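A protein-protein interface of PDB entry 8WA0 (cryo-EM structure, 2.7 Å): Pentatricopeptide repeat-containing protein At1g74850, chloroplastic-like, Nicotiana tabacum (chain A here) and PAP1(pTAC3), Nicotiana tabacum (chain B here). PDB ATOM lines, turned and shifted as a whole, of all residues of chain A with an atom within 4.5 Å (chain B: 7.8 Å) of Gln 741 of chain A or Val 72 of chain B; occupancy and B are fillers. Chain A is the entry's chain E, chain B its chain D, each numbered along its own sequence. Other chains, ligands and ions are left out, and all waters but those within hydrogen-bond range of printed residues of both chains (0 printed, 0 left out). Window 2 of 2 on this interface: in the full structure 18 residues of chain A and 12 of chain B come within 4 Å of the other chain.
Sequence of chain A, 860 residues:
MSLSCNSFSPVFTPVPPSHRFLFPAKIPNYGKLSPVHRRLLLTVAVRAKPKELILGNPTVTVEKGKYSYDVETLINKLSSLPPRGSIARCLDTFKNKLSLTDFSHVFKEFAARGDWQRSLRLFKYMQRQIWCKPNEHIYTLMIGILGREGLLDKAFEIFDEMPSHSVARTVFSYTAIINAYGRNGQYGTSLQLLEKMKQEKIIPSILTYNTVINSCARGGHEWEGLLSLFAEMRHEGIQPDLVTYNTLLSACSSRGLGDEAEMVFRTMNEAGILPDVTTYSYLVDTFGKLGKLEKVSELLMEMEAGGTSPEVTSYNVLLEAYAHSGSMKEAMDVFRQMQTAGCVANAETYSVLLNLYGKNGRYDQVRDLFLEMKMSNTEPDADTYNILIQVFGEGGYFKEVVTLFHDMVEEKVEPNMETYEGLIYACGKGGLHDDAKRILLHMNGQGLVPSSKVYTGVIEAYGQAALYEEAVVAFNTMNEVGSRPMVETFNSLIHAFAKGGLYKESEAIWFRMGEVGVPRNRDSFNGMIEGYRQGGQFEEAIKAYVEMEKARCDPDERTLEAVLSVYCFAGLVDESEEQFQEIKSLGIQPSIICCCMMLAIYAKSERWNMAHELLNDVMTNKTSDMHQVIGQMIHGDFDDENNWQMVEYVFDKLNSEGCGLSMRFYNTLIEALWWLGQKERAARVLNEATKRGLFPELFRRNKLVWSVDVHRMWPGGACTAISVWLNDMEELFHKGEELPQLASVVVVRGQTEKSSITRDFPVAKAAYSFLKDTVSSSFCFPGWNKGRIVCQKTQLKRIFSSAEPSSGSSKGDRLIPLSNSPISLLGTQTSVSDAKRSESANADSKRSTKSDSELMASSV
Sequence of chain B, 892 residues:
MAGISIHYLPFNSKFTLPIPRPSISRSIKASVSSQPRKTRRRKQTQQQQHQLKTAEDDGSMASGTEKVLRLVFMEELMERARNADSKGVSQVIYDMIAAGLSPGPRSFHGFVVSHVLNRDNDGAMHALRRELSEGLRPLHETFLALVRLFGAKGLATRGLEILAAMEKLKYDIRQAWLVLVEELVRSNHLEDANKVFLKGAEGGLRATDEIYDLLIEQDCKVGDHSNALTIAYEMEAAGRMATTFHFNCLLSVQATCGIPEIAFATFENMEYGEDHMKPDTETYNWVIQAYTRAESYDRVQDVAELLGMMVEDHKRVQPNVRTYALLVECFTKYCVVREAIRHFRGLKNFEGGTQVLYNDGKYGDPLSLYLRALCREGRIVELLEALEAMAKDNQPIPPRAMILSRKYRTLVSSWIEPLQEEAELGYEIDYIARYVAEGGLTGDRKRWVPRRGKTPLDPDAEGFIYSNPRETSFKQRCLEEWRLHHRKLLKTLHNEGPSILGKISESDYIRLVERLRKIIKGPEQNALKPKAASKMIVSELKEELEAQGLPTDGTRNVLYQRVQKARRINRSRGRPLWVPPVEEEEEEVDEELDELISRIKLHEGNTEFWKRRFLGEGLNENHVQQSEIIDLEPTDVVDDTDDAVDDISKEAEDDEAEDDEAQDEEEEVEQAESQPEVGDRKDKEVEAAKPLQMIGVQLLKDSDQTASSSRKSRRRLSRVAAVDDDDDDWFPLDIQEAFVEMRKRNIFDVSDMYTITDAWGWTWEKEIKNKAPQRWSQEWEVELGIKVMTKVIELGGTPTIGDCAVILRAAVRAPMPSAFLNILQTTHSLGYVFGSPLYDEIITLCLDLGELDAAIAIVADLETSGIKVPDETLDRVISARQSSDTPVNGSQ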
ATOM      1  N   LYS A 703     -17.886  -7.774 -24.065  1.00  0.00           N
ATOM      2  CA  LYS A 703     -17.684  -7.556 -22.637  1.00  0.00           C
ATOM      3  C   LYS A 703     -16.820  -8.652 -22.027  1.00  0.00           C
ATOM      4  O   LYS A 703     -15.964  -8.377 -21.179  1.00  0.00           O
ATOM      5  CB  LYS A 703     -19.033  -7.473 -21.923  1.00  0.00           C
ATOM      6  CG  LYS A 703     -18.933  -7.374 -20.409  1.00  0.00           C
ATOM      7  CD  LYS A 703     -18.162  -6.133 -19.985  1.00  0.00           C
ATOM      8  CE  LYS A 703     -17.986  -6.084 -18.476  1.00  0.00           C
ATOM      9  NZ  LYS A 703     -19.293  -6.086 -17.763  1.00  0.00           N
ATOM     10  N   LEU A 704     -17.024  -9.900 -22.451  1.00  0.00           N
ATOM     11  CA  LEU A 704     -16.283 -11.011 -21.866  1.00  0.00           C
ATOM     12  C   LEU A 704     -14.954 -11.245 -22.570  1.00  0.00           C
ATOM     13  O   LEU A 704     -13.944 -11.529 -21.915  1.00  0.00           O
ATOM     14  CB  LEU A 704     -17.130 -12.287 -21.898  1.00  0.00           C
ATOM     15  CG  LEU A 704     -17.645 -12.781 -23.252  1.00  0.00           C
ATOM     16  CD1 LEU A 704     -17.678 -14.301 -23.291  1.00  0.00           C
ATOM     17  CD2 LEU A 704     -19.025 -12.213 -23.553  1.00  0.00           C
ATOM     18  N   LEU A 739     -11.581  -3.936 -18.737  1.00  0.00           N
ATOM     19  CA  LEU A 739     -10.730  -4.825 -19.510  1.00  0.00           C
ATOM     20  C   LEU A 739     -11.362  -6.212 -19.619  1.00  0.00           C
ATOM     21  O   LEU A 739     -12.105  -6.637 -18.728  1.00  0.00           O
ATOM     22  CB  LEU A 739      -9.348  -4.924 -18.869  1.00  0.00           C
ATOM     23  CG  LEU A 739      -9.271  -5.100 -17.349  1.00  0.00           C
ATOM     24  CD1 LEU A 739      -9.328  -6.568 -16.944  1.00  0.00           C
ATOM     25  CD2 LEU A 739      -8.017  -4.436 -16.803  1.00  0.00           C
ATOM     26  N   PRO A 740     -11.088  -6.934 -20.703  1.00  0.00           N
ATOM     27  CA  PRO A 740     -11.677  -8.265 -20.869  1.00  0.00           C
ATOM     28  C   PRO A 740     -11.083  -9.269 -19.894  1.00  0.00           C
ATOM     29  O   PRO A 740      -9.999  -9.080 -19.339  1.00  0.00           O
ATOM     30  CB  PRO A 740     -11.329  -8.627 -22.316  1.00  0.00           C
ATOM     31  CG  PRO A 740     -10.080  -7.858 -22.589  1.00  0.00           C
ATOM     32  CD  PRO A 740     -10.245  -6.559 -21.851  1.00  0.00           C
ATOM     33  N   GLN A 741     -11.824 -10.361 -19.692  1.00  0.00           N
ATOM     34  CA  GLN A 741     -11.346 -11.419 -18.809  1.00  0.00           C
ATOM     35  C   GLN A 741     -10.225 -12.222 -19.453  1.00  0.00           C
ATOM     36  O   GLN A 741      -9.369 -12.764 -18.744  1.00  0.00           O
ATOM     37  CB  GLN A 741     -12.502 -12.342 -18.415  1.00  0.00           C
ATOM     38  CG  GLN A 741     -13.465 -11.752 -17.391  1.00  0.00           C
ATOM     39  CD  GLN A 741     -14.353 -10.664 -17.967  1.00  0.00           C
ATOM     40  OE1 GLN A 741     -14.406 -10.468 -19.183  1.00  0.00           O
ATOM     41  NE2 GLN A 741     -15.057  -9.952 -17.096  1.00  0.00           N
ATOM     42  N   LEU A 742     -10.208 -12.310 -20.781  1.00  0.00           N
ATOM     43  CA  LEU A 742      -9.175 -13.060 -21.488  1.00  0.00           C
ATOM     44  C   LEU A 742      -9.008 -12.468 -22.877  1.00  0.00           C
ATOM     45  O   LEU A 742      -9.973 -12.404 -23.644  1.00  0.00           O
ATOM     46  CB  LEU A 742      -9.536 -14.544 -21.575  1.00  0.00           C
ATOM     47  CG  LEU A 742      -8.473 -15.471 -22.166  1.00  0.00           C
ATOM     48  CD1 LEU A 742      -7.248 -15.514 -21.269  1.00  0.00           C
ATOM     49  CD2 LEU A 742      -9.035 -16.868 -22.379  1.00  0.00           C
ATOM     50  N   ALA A 743      -7.791 -12.038 -23.197  1.00  0.00           N
ATOM     51  CA  ALA A 743      -7.463 -11.502 -24.512  1.00  0.00           C
ATOM     52  C   ALA A 743      -6.667 -12.549 -25.281  1.00  0.00           C
ATOM     53  O   ALA A 743      -5.543 -12.886 -24.894  1.00  0.00           O
ATOM     54  CB  ALA A 743      -6.674 -10.199 -24.392  1.00  0.00           C
ATOM     55  N   GLN A 792      -3.885 -12.906 -19.436  1.00  0.00           N
ATOM     56  CA  GLN A 792      -4.832 -12.748 -18.341  1.00  0.00           C
ATOM     57  C   GLN A 792      -5.144 -11.288 -18.072  1.00  0.00           C
ATOM     58  O   GLN A 792      -4.368 -10.405 -18.432  1.00  0.00           O
ATOM     59  CB  GLN A 792      -4.330 -13.438 -17.072  1.00  0.00           C
ATOM     60  CG  GLN A 792      -4.085 -14.929 -17.239  1.00  0.00           C
ATOM     61  CD  GLN A 792      -5.353 -15.714 -17.518  1.00  0.00           C
ATOM     62  OE1 GLN A 792      -5.337 -16.686 -18.274  1.00  0.00           O
ATOM     63  NE2 GLN A 792      -6.459 -15.296 -16.911  1.00  0.00           N
ATOM     64  N   LYS A 793      -6.277 -11.027 -17.426  1.00  0.00           N
ATOM     65  CA  LYS A 793      -6.704  -9.653 -17.144  1.00  0.00           C
ATOM     66  C   LYS A 793      -5.683  -8.788 -16.410  1.00  0.00           C
ATOM     67  O   LYS A 793      -5.320  -7.709 -16.879  1.00  0.00           O
ATOM     68  CB  LYS A 793      -8.007  -9.692 -16.354  1.00  0.00           C
ATOM     69  CG  LYS A 793      -8.325 -11.049 -15.752  1.00  0.00           C
ATOM     70  CD  LYS A 793      -9.721 -11.067 -15.154  1.00  0.00           C
ATOM     71  CE  LYS A 793     -10.103 -12.465 -14.698  1.00  0.00           C
ATOM     72  NZ  LYS A 793     -11.488 -12.510 -14.153  1.00  0.00           N
ATOM     73  N   THR B  65      -6.641 -20.555 -13.941  1.00  0.00           N
ATOM     74  CA  THR B  65      -7.010 -19.386 -14.724  1.00  0.00           C
ATOM     75  C   THR B  65      -8.167 -19.719 -15.651  1.00  0.00           C
ATOM     76  O   THR B  65      -9.097 -18.928 -15.790  1.00  0.00           O
ATOM     77  CB  THR B  65      -5.827 -18.863 -15.552  1.00  0.00           C
ATOM     78  N   GLU B  66      -8.140 -20.912 -16.243  1.00  0.00           N
ATOM     79  CA  GLU B  66      -9.187 -21.308 -17.154  1.00  0.00           C
ATOM     80  C   GLU B  66     -10.451 -21.273 -16.390  1.00  0.00           C
ATOM     81  O   GLU B  66     -11.472 -20.883 -16.908  1.00  0.00           O
ATOM     82  CB  GLU B  66      -8.959 -22.718 -17.654  1.00  0.00           C
ATOM     83  N   LYS B  67     -10.398 -21.689 -15.143  1.00  0.00           N
ATOM     84  CA  LYS B  67     -11.604 -21.763 -14.379  1.00  0.00           C
ATOM     85  C   LYS B  67     -12.200 -20.406 -14.216  1.00  0.00           C
ATOM     86  O   LYS B  67     -13.400 -20.240 -14.371  1.00  0.00           O
ATOM     87  CB  LYS B  67     -11.317 -22.350 -13.003  1.00  0.00           C
ATOM     88  N   VAL B  68     -11.383 -19.417 -13.923  1.00  0.00           N
ATOM     89  CA  VAL B  68     -11.964 -18.133 -13.653  1.00  0.00           C
ATOM     90  C   VAL B  68     -12.629 -17.639 -14.884  1.00  0.00           C
ATOM     91  O   VAL B  68     -13.747 -17.154 -14.842  1.00  0.00           O
ATOM     92  CB  VAL B  68     -10.891 -17.132 -13.233  1.00  0.00           C
ATOM     93  N   LEU B  69     -11.937 -17.772 -16.007  1.00  0.00           N
ATOM     94  CA  LEU B  69     -12.502 -17.336 -17.282  1.00  0.00           C
ATOM     95  C   LEU B  69     -13.696 -18.146 -17.770  1.00  0.00           C
ATOM     96  O   LEU B  69     -14.656 -17.594 -18.292  1.00  0.00           O
ATOM     97  CB  LEU B  69     -11.428 -17.188 -18.370  1.00  0.00           C
ATOM     98  N   ARG B  70     -13.644 -19.461 -17.617  1.00  0.00           N
ATOM     99  CA  ARG B  70     -14.723 -20.247 -18.117  1.00  0.00           C
ATOM    100  C   ARG B  70     -15.903 -19.807 -17.323  1.00  0.00           C
ATOM    101  O   ARG B  70     -16.963 -19.545 -17.873  1.00  0.00           O
ATOM    102  CB  ARG B  70     -14.464 -21.748 -17.971  1.00  0.00           C
ATOM    103  N   LEU B  71     -15.703 -19.629 -16.033  1.00  0.00           N
ATOM    104  CA  LEU B  71     -16.788 -19.230 -15.179  1.00  0.00           C
ATOM    105  C   LEU B  71     -17.357 -17.886 -15.536  1.00  0.00           C
ATOM    106  O   LEU B  71     -18.575 -17.703 -15.564  1.00  0.00           O
ATOM    107  CB  LEU B  71     -16.328 -19.211 -13.730  1.00  0.00           C
ATOM    108  N   VAL B  72     -16.485 -16.930 -15.821  1.00  0.00           N
ATOM    109  CA  VAL B  72     -16.961 -15.604 -16.210  1.00  0.00           C
ATOM    110  C   VAL B  72     -17.709 -15.598 -17.526  1.00  0.00           C
ATOM    111  O   VAL B  72     -18.713 -14.901 -17.657  1.00  0.00           O
ATOM    112  CB  VAL B  72     -15.884 -14.512 -16.200  1.00  0.00           C
ATOM    113  N   PHE B  73     -17.237 -16.357 -18.501  1.00  0.00           N
ATOM    114  CA  PHE B  73     -17.915 -16.304 -19.769  1.00  0.00           C
ATOM    115  C   PHE B  73     -19.321 -16.814 -19.640  1.00  0.00           C
ATOM    116  O   PHE B  73     -20.265 -16.178 -20.082  1.00  0.00           O
ATOM    117  CB  PHE B  73     -17.193 -17.180 -20.795  1.00  0.00           C
ATOM    118  N   MET B  74     -19.479 -17.918 -18.938  1.00  0.00           N
ATOM    119  CA  MET B  74     -20.774 -18.556 -18.888  1.00  0.00           C
ATOM    120  C   MET B  74     -21.858 -17.738 -18.294  1.00  0.00           C
ATOM    121  O   MET B  74     -23.007 -17.861 -18.705  1.00  0.00           O
ATOM    122  CB  MET B  74     -20.692 -19.903 -18.194  1.00  0.00           C
ATOM    123  N   GLU B  75     -21.542 -16.909 -17.323  1.00  0.00           N
ATOM    124  CA  GLU B  75     -22.602 -16.189 -16.659  1.00  0.00           C
ATOM    125  C   GLU B  75     -23.285 -15.388 -17.727  1.00  0.00           C
ATOM    126  O   GLU B  75     -24.502 -15.200 -17.705  1.00  0.00           O
ATOM    127  CB  GLU B  75     -22.058 -15.277 -15.586  1.00  0.00           C
ATOM    128  N   GLU B  76     -22.498 -14.895 -18.670  1.00  0.00           N
ATOM    129  CA  GLU B  76     -23.075 -14.143 -19.756  1.00  0.00           C
ATOM    130  C   GLU B  76     -24.001 -14.926 -20.649  1.00  0.00           C
ATOM    131  O   GLU B  76     -25.054 -14.428 -21.025  1.00  0.00           O
ATOM    132  CB  GLU B  76     -21.966 -13.528 -20.607  1.00  0.00           C
ATOM    133  N   LEU B  77     -23.645 -16.148 -20.992  1.00  0.00           N
ATOM    134  CA  LEU B  77     -24.452 -16.859 -21.958  1.00  0.00           C
ATOM    135  C   LEU B  77     -25.775 -16.990 -21.352  1.00  0.00           C
ATOM    136  O   LEU B  77     -26.797 -16.775 -21.977  1.00  0.00           O
ATOM    137  CB  LEU B  77     -23.866 -18.234 -22.226  1.00  0.00           C
ATOM    138  N   ALA B  99     -11.365 -16.899 -27.837  1.00  0.00           N
ATOM    139  CA  ALA B  99     -10.638 -17.002 -26.605  1.00  0.00           C
ATOM    140  C   ALA B  99      -9.974 -18.333 -26.625  1.00  0.00           C
ATOM    141  O   ALA B  99      -8.992 -18.541 -25.924  1.00  0.00           O
ATOM    142  CB  ALA B  99     -11.585 -16.910 -25.429  1.00  0.00           C
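The backbone carbonyl oxygen of Lys 703 of chain A sits close to the side-chain amide oxygen of Gln 741 of chain A (3.3 Å). O of Leu 704 of chain A lies close to OE1 of Gln 741 of chain A, at 3.0 Å.
CD1 of Leu 704 of chain A touches CB of Phe 73 of chain B (3.8 Å). Val 72 of chain B touches Gln 741 of chain A (CB to CG, 3.9 Å). Leu 742 of chain A touches Ala 99 of chain B. OE1 of Gln 792 of chain A touches CB of Thr 65 of chain B (3.5 Å).
Of the printed residues of chain B, Gln 741 of chain A touches Val 72. Val 72 of chain B touches just one residue of chain A: Gln 741 (3.9 Å). Of the printed residues of chain B, Leu 704 of chain A touches Phe 73 (3.8 Å). Of the printed residues of chain A, Ala 99 of chain B touches Leu 742. Printed residues of chain A within 4 Å of Thr 65 of chain B: Gln 792. Leu 739 of chain A touches none of the printed residues of chain B.
Printed residues of chain B that touch a printed residue of chain A: Thr 65, Val 72, Phe 73 and Ala 99. Hydrophobic or aromatic side chains of chain B within 4 Å of the printed part of chain A: Val 72, Phe 73 and Ala 99. Along chain B the printed residues that touch a printed residue of chain A span positions 65 to 99. Of the 9 printed residues of chain A, 4 touch a printed residue of chain B. Hydrophobic or aromatic side chains of chain A within 4 Å of the printed part of chain B: Leu 704 and Leu 742.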
